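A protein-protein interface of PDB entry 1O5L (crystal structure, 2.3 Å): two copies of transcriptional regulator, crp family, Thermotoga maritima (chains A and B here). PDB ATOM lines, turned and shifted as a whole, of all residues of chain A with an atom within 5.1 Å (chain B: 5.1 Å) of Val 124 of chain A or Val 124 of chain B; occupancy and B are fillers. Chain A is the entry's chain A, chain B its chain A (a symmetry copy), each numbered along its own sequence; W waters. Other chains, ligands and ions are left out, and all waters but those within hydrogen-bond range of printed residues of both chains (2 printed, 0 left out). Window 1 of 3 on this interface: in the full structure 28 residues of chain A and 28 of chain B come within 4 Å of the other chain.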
ATOM      1  N   SER A  76      -0.504  23.036  -3.718  1.00  0.00           N
ATOM      2  CA  SER A  76      -0.010  22.178  -4.788  1.00  0.00           C
ATOM      3  C   SER A  76       1.473  21.798  -4.634  1.00  0.00           C
ATOM      4  O   SER A  76       1.871  20.640  -4.835  1.00  0.00           O
ATOM      5  CB  SER A  76      -0.307  22.845  -6.156  1.00  0.00           C
ATOM      6  OG  SER A  76       0.587  23.915  -6.452  1.00  0.00           O
ATOM      7  N   GLY A  77       2.290  22.772  -4.288  1.00  0.00           N
ATOM      8  CA  GLY A  77       3.717  22.529  -4.044  1.00  0.00           C
ATOM      9  C   GLY A  77       4.086  21.650  -2.839  1.00  0.00           C
ATOM     10  O   GLY A  77       5.241  21.274  -2.692  1.00  0.00           O
ATOM     11  N   PHE A 120      -0.068  21.370 -14.019  1.00  0.00           N
ATOM     12  CA  PHE A 120       0.397  21.084 -12.659  1.00  0.00           C
ATOM     13  C   PHE A 120       1.845  21.531 -12.409  1.00  0.00           C
ATOM     14  O   PHE A 120       2.136  22.184 -11.395  1.00  0.00           O
ATOM     15  CB  PHE A 120       0.262  19.570 -12.342  1.00  0.00           C
ATOM     16  CG  PHE A 120       0.573  19.227 -10.902  1.00  0.00           C
ATOM     17  CD1 PHE A 120      -0.255  19.667  -9.885  1.00  0.00           C
ATOM     18  CD2 PHE A 120       1.706  18.539 -10.567  1.00  0.00           C
ATOM     19  CE1 PHE A 120       0.021  19.406  -8.570  1.00  0.00           C
ATOM     20  CE2 PHE A 120       1.993  18.259  -9.214  1.00  0.00           C
ATOM     21  CZ  PHE A 120       1.131  18.701  -8.231  1.00  0.00           C
ATOM     22  N   LEU A 121       2.764  21.163 -13.298  1.00  0.00           N
ATOM     23  CA  LEU A 121       4.153  21.542 -13.106  1.00  0.00           C
ATOM     24  C   LEU A 121       4.300  23.087 -13.160  1.00  0.00           C
ATOM     25  O   LEU A 121       5.080  23.651 -12.374  1.00  0.00           O
ATOM     26  CB  LEU A 121       5.067  20.875 -14.115  1.00  0.00           C
ATOM     27  CG  LEU A 121       5.241  19.356 -14.074  1.00  0.00           C
ATOM     28  CD1 LEU A 121       6.103  18.946 -15.264  1.00  0.00           C
ATOM     29  CD2 LEU A 121       5.860  18.852 -12.757  1.00  0.00           C
ATOM     30  N   LYS A 122       3.526  23.739 -14.053  1.00  0.00           N
ATOM     31  CA  LYS A 122       3.434  25.199 -14.126  1.00  0.00           C
ATOM     32  C   LYS A 122       2.903  25.846 -12.833  1.00  0.00           C
ATOM     33  O   LYS A 122       3.432  26.862 -12.371  1.00  0.00           O
ATOM     34  CB  LYS A 122       2.556  25.625 -15.315  1.00  0.00           C
ATOM     35  CG  LYS A 122       2.581  27.138 -15.640  1.00  0.00           C
ATOM     36  CD  LYS A 122       1.710  27.507 -16.880  1.00  0.00           C
ATOM     37  CE  LYS A 122       1.661  29.044 -17.073  1.00  0.00           C
ATOM     38  NZ  LYS A 122       1.143  29.509 -18.426  1.00  0.00           N
ATOM     39  N   ASP A 123       1.868  25.250 -12.254  1.00  0.00           N
ATOM     40  CA  ASP A 123       1.280  25.743 -11.007  1.00  0.00           C
ATOM     41  C   ASP A 123       2.290  25.723  -9.849  1.00  0.00           C
ATOM     42  O   ASP A 123       2.445  26.705  -9.109  1.00  0.00           O
ATOM     43  CB  ASP A 123       0.072  24.885 -10.644  1.00  0.00           C
ATOM     44  CG  ASP A 123      -0.658  25.371  -9.409  1.00  0.00           C
ATOM     45  OD1 ASP A 123      -0.263  25.216  -8.247  1.00  0.00           O
ATOM     46  OD2 ASP A 123      -1.728  25.951  -9.544  1.00  0.00           O
ATOM     47  N   VAL A 124       2.961  24.594  -9.709  1.00  0.00           N
ATOM     48  CA  VAL A 124       3.948  24.407  -8.666  1.00  0.00           C
ATOM     49  C   VAL A 124       5.164  25.337  -8.863  1.00  0.00           C
ATOM     50  O   VAL A 124       5.653  25.936  -7.877  1.00  0.00           O
ATOM     51  CB  VAL A 124       4.388  22.917  -8.575  1.00  0.00           C
ATOM     52  CG1 VAL A 124       5.546  22.752  -7.646  1.00  0.00           C
ATOM     53  CG2 VAL A 124       3.224  22.071  -8.119  1.00  0.00           C
ATOM     54  N   SER A 125       5.638  25.459 -10.112  1.00  0.00           N
ATOM     55  CA  SER A 125       6.788  26.317 -10.421  1.00  0.00           C
ATOM     56  C   SER A 125       6.543  27.818 -10.233  1.00  0.00           C
ATOM     57  O   SER A 125       7.437  28.550  -9.797  1.00  0.00           O
ATOM     58  CB  SER A 125       7.303  26.047 -11.826  1.00  0.00           C
ATOM     59  OG  SER A 125       7.540  24.655 -11.952  1.00  0.00           O
ATOM     60  N   GLU A 126       5.354  28.265 -10.601  1.00  0.00           N
ATOM     61  CA  GLU A 126       4.948  29.661 -10.414  1.00  0.00           C
ATOM     62  C   GLU A 126       4.843  30.022  -8.937  1.00  0.00           C
ATOM     63  O   GLU A 126       5.251  31.107  -8.530  1.00  0.00           O
ATOM     64  CB  GLU A 126       3.621  29.965 -11.148  1.00  0.00           C
ATOM     65  CG  GLU A 126       3.791  30.253 -12.634  1.00  0.00           C
ATOM     66  CD  GLU A 126       4.729  31.421 -12.850  1.00  0.00           C
ATOM     67  OE1 GLU A 126       4.373  32.537 -12.438  1.00  0.00           O
ATOM     68  OE2 GLU A 126       5.847  31.221 -13.373  1.00  0.00           O
ATOM     69  N   HIS A 127       4.322  29.101  -8.128  1.00  0.00           N
ATOM     70  CA  HIS A 127       4.263  29.326  -6.685  1.00  0.00           C
ATOM     71  C   HIS A 127       5.650  29.342  -6.080  1.00  0.00           C
ATOM     72  O   HIS A 127       5.921  30.092  -5.152  1.00  0.00           O
ATOM     73  CB  HIS A 127       3.372  28.285  -5.983  1.00  0.00           C
ATOM     74  CG  HIS A 127       1.911  28.595  -6.061  1.00  0.00           C
ATOM     75  ND1 HIS A 127       1.060  27.955  -6.936  1.00  0.00           N
ATOM     76  CD2 HIS A 127       1.158  29.511  -5.408  1.00  0.00           C
ATOM     77  CE1 HIS A 127      -0.156  28.455  -6.811  1.00  0.00           C
ATOM     78  NE2 HIS A 127      -0.124  29.399  -5.891  1.00  0.00           N
ATOM     79  N   PHE A 128       6.513  28.467  -6.582  1.00  0.00           N
ATOM     80  CA  PHE A 128       7.897  28.438  -6.150  1.00  0.00           C
ATOM     81  C   PHE A 128       8.639  29.746  -6.472  1.00  0.00           C
ATOM     82  O   PHE A 128       9.349  30.273  -5.644  1.00  0.00           O
ATOM     83  CB  PHE A 128       8.630  27.282  -6.797  1.00  0.00           C
ATOM     84  CG  PHE A 128      10.045  27.121  -6.322  1.00  0.00           C
ATOM     85  CD1 PHE A 128      10.334  26.960  -4.988  1.00  0.00           C
ATOM     86  CD2 PHE A 128      11.091  27.160  -7.200  1.00  0.00           C
ATOM     87  CE1 PHE A 128      11.637  26.803  -4.559  1.00  0.00           C
ATOM     88  CE2 PHE A 128      12.401  27.006  -6.752  1.00  0.00           C
ATOM     89  CZ  PHE A 128      12.659  26.820  -5.446  1.00  0.00           C
ATOM     90  N   SER B  76      15.465  22.859 -10.447  1.00  0.00           N
ATOM     91  CA  SER B  76      14.350  21.992 -10.805  1.00  0.00           C
ATOM     92  C   SER B  76      12.979  22.682 -10.703  1.00  0.00           C
ATOM     93  O   SER B  76      12.113  22.537 -11.579  1.00  0.00           O
ATOM     94  CB  SER B  76      14.420  20.694  -9.959  1.00  0.00           C
ATOM     95  OG  SER B  76      13.981  20.887  -8.617  1.00  0.00           O
ATOM     96  N   GLY B  77      12.776  23.420  -9.631  1.00  0.00           N
ATOM     97  CA  GLY B  77      11.538  24.184  -9.444  1.00  0.00           C
ATOM     98  C   GLY B  77      11.268  25.340 -10.419  1.00  0.00           C
ATOM     99  O   GLY B  77      10.178  25.894 -10.420  1.00  0.00           O
ATOM    100  N   PHE B 120      11.048  13.464  -9.301  1.00  0.00           N
ATOM    101  CA  PHE B 120      10.983  14.861  -9.743  1.00  0.00           C
ATOM    102  C   PHE B 120      10.001  15.708  -8.920  1.00  0.00           C
ATOM    103  O   PHE B 120      10.343  16.816  -8.478  1.00  0.00           O
ATOM    104  CB  PHE B 120      10.602  14.941 -11.245  1.00  0.00           C
ATOM    105  CG  PHE B 120      10.672  16.343 -11.809  1.00  0.00           C
ATOM    106  CD1 PHE B 120      11.890  16.988 -11.929  1.00  0.00           C
ATOM    107  CD2 PHE B 120       9.539  17.028 -12.147  1.00  0.00           C
ATOM    108  CE1 PHE B 120      11.982  18.270 -12.398  1.00  0.00           C
ATOM    109  CE2 PHE B 120       9.626  18.348 -12.639  1.00  0.00           C
ATOM    110  CZ  PHE B 120      10.862  18.948 -12.760  1.00  0.00           C
ATOM    111  N   LEU B 121       8.776  15.224  -8.737  1.00  0.00           N
ATOM    112  CA  LEU B 121       7.797  15.990  -7.982  1.00  0.00           C
ATOM    113  C   LEU B 121       8.266  16.155  -6.511  1.00  0.00           C
ATOM    114  O   LEU B 121       8.080  17.240  -5.933  1.00  0.00           O
ATOM    115  CB  LEU B 121       6.419  15.363  -8.043  1.00  0.00           C
ATOM    116  CG  LEU B 121       5.679  15.314  -9.381  1.00  0.00           C
ATOM    117  CD1 LEU B 121       4.389  14.529  -9.182  1.00  0.00           C
ATOM    118  CD2 LEU B 121       5.382  16.710  -9.962  1.00  0.00           C
ATOM    119  N   LYS B 122       8.896  15.101  -5.952  1.00  0.00           N
ATOM    120  CA  LYS B 122       9.529  15.147  -4.632  1.00  0.00           C
ATOM    121  C   LYS B 122      10.666  16.182  -4.532  1.00  0.00           C
ATOM    122  O   LYS B 122      10.767  16.917  -3.546  1.00  0.00           O
ATOM    123  CB  LYS B 122      10.060  13.758  -4.240  1.00  0.00           C
ATOM    124  CG  LYS B 122      10.532  13.625  -2.772  1.00  0.00           C
ATOM    125  CD  LYS B 122      11.018  12.186  -2.418  1.00  0.00           C
ATOM    126  CE  LYS B 122      11.607  12.148  -0.985  1.00  0.00           C
ATOM    127  NZ  LYS B 122      11.791  10.755  -0.400  1.00  0.00           N
ATOM    128  N   ASP B 123      11.507  16.239  -5.558  1.00  0.00           N
ATOM    129  CA  ASP B 123      12.617  17.194  -5.608  1.00  0.00           C
ATOM    130  C   ASP B 123      12.122  18.649  -5.577  1.00  0.00           C
ATOM    131  O   ASP B 123      12.622  19.486  -4.812  1.00  0.00           O
ATOM    132  CB  ASP B 123      13.431  16.958  -6.875  1.00  0.00           C
ATOM    133  CG  ASP B 123      14.655  17.845  -6.973  1.00  0.00           C
ATOM    134  OD1 ASP B 123      14.636  19.046  -7.270  1.00  0.00           O
ATOM    135  OD2 ASP B 123      15.756  17.356  -6.763  1.00  0.00           O
ATOM    136  N   VAL B 124      11.145  18.927  -6.421  1.00  0.00           N
ATOM    137  CA  VAL B 124      10.567  20.252  -6.523  1.00  0.00           C
ATOM    138  C   VAL B 124       9.829  20.648  -5.227  1.00  0.00           C
ATOM    139  O   VAL B 124       9.971  21.803  -4.762  1.00  0.00           O
ATOM    140  CB  VAL B 124       9.630  20.356  -7.760  1.00  0.00           C
ATOM    141  CG1 VAL B 124       8.876  21.646  -7.758  1.00  0.00           C
ATOM    142  CG2 VAL B 124      10.442  20.224  -9.026  1.00  0.00           C
ATOM    143  N   SER B 125       9.061  19.709  -4.654  1.00  0.00           N
ATOM    144  CA  SER B 125       8.313  19.971  -3.418  1.00  0.00           C
ATOM    145  C   SER B 125       9.181  20.198  -2.176  1.00  0.00           C
ATOM    146  O   SER B 125       8.849  21.026  -1.321  1.00  0.00           O
ATOM    147  CB  SER B 125       7.305  18.866  -3.152  1.00  0.00           C
ATOM    148  OG  SER B 125       6.508  18.703  -4.312  1.00  0.00           O
ATOM    149  N   GLU B 126      10.257  19.437  -2.068  1.00  0.00           N
ATOM    150  CA  GLU B 126      11.220  19.589  -0.974  1.00  0.00           C
ATOM    151  C   GLU B 126      11.938  20.931  -1.041  1.00  0.00           C
ATOM    152  O   GLU B 126      12.153  21.576  -0.017  1.00  0.00           O
ATOM    153  CB  GLU B 126      12.237  18.424  -0.952  1.00  0.00           C
ATOM    154  CG  GLU B 126      11.718  17.166  -0.269  1.00  0.00           C
ATOM    155  CD  GLU B 126      11.306  17.460   1.156  1.00  0.00           C
ATOM    156  OE1 GLU B 126      12.190  17.808   1.957  1.00  0.00           O
ATOM    157  OE2 GLU B 126      10.098  17.406   1.469  1.00  0.00           O
ATOM    158  N   HIS B 127      12.286  21.370  -2.249  1.00  0.00           N
ATOM    159  CA  HIS B 127      12.899  22.685  -2.418  1.00  0.00           C
ATOM    160  C   HIS B 127      11.914  23.789  -2.095  1.00  0.00           C
ATOM    161  O   HIS B 127      12.284  24.820  -1.548  1.00  0.00           O
ATOM    162  CB  HIS B 127      13.480  22.866  -3.832  1.00  0.00           C
ATOM    163  CG  HIS B 127      14.829  22.247  -4.009  1.00  0.00           C
ATOM    164  ND1 HIS B 127      15.018  21.047  -4.658  1.00  0.00           N
ATOM    165  CD2 HIS B 127      16.053  22.638  -3.580  1.00  0.00           C
ATOM    166  CE1 HIS B 127      16.301  20.728  -4.631  1.00  0.00           C
ATOM    167  NE2 HIS B 127      16.948  21.677  -3.985  1.00  0.00           N
ATOM    168  N   PHE B 128      10.662  23.584  -2.486  1.00  0.00           N
ATOM    169  CA  PHE B 128       9.606  24.525  -2.164  1.00  0.00           C
ATOM    170  C   PHE B 128       9.384  24.659  -0.649  1.00  0.00           C
ATOM    171  O   PHE B 128       9.255  25.750  -0.139  1.00  0.00           O
ATOM    172  CB  PHE B 128       8.308  24.106  -2.821  1.00  0.00           C
ATOM    173  CG  PHE B 128       7.186  25.084  -2.619  1.00  0.00           C
ATOM    174  CD1 PHE B 128       7.312  26.400  -2.998  1.00  0.00           C
ATOM    175  CD2 PHE B 128       6.017  24.703  -2.026  1.00  0.00           C
ATOM    176  CE1 PHE B 128       6.275  27.292  -2.819  1.00  0.00           C
ATOM    177  CE2 PHE B 128       4.980  25.616  -1.846  1.00  0.00           C
ATOM    178  CZ  PHE B 128       5.114  26.889  -2.251  1.00  0.00           C
HETATM  179  O   HOH W   1       9.805  23.077 -12.721  1.00  0.00           O
HETATM  180  O   HOH W   2       3.687  18.739  -4.821  1.00  0.00           O
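The backbone carbonyl oxygen (O) of Gly 77 of chain A lies close to the side-chain hydroxyl (OG) of Ser 125 of chain B (3.3 Å). The side-chain hydroxyl (OG) of Ser 125 of chain A sits close to the backbone carbonyl oxygen (O) of Gly 77 of chain B (3.3 Å).
The backbone carbonyl oxygen (O) of Leu 121 of chain A lies within hydrogen-bond range of the side-chain hydroxyl (OG) of Ser 125 of chain A. The backbone carbonyl oxygen (O) of Asp 123 of chain A lies within hydrogen-bond range of a ring nitrogen (ND1) of His 127 of chain A. O of Leu 121 of chain B sits at hydrogen-bond distance from OG of Ser 125 of chain B (2.7 Å). ND1 of His 127 of chain B is in hydrogen-bond range of O of Asp 123 of chain B.
Phe 128 of chain B touches Gly 77 of chain A. CE2 of Phe 120 of chain A touches CD2 of Leu 121 of chain B, 3.8 Å away. Leu 121 of chain A touches Phe 120 of chain B (CD2 to CE2, 3.8 Å). Leu 121 of chain A touches Leu 121 of chain B. Val 124 of chain A touches Val 124 of chain B (CG1 to CG1, 3.5 Å). His 127 of chain A touches Phe 128 of chain B (O to CE1, 3.7 Å). Phe 128 of chain A touches Gly 77 of chain B (CD2 to O, 3.6 Å). O of His 127 of chain B touches CE1 of Phe 128 of chain A, at 3.7 Å. Phe 128 of chain A touches Phe 128 of chain B (CD1 to CD1, 3.7 Å).
Of chain B, only Val 124 (3.5 Å) comes within 4 Å of Val 124 of chain A. Val 124 of chain B touches just one residue of chain A: Val 124. Of the printed residues of chain A, Phe 120 of chain B touches Leu 121 (3.8 Å). Of the printed residues of chain B, Gly 77 of chain A touches Ser 125 and Phe 128. Of the printed residues of chain A, Gly 77 of chain B touches Ser 125 (3.2 Å) and Phe 128 (3.6 Å). Printed residues of chain A within 4 Å of His 127 of chain B: Phe 128 (3.7 Å).
Of the 11 printed residues of chain B, 7 touch a printed residue of chain A. Printed residues of chain A that touch a printed residue of chain B: Gly 77, Phe 120, Leu 121, Val 124, Ser 125, His 127 and Phe 128. Along chain A the printed residues that touch a printed residue of chain B span positions 77 to 128. Among the printed residues, 11 pairs touch across the chains. Among the printed residues, no Asp or Glu carboxylate lies within 4 Å of a Lys or Arg side-chain nitrogen of the other chain.
Gly 77 of chain A touches Ser 125 of chain B, and with the chains exchanged Ser 125 of chain A touches Gly 77 of chain B. Phe 120 of chain A touches Leu 121 of chain B, and with the chains exchanged Leu 121 of chain A touches Phe 120 of chain B. Val 124 of chain B touches its own counterpart, Val 124 of chain A. His 127 of chain A touches Phe 128 of chain B, and with the chains exchanged Phe 128 of chain A touches His 127 of chain B. 11 positions are printed for both chains. Of the 11 pairs that touch across the chains among the printed residues, 11 have their exchanged pair printed and touching as well.
Water W2 bridges O of Ser 76 of chain A (2.6 Å) and OG of Ser 125 of chain B (2.9 Å). Water W1 bridges O of Ser 76 of chain B (2.6 Å) and OG of Ser 125 of chain A (2.9 Å).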
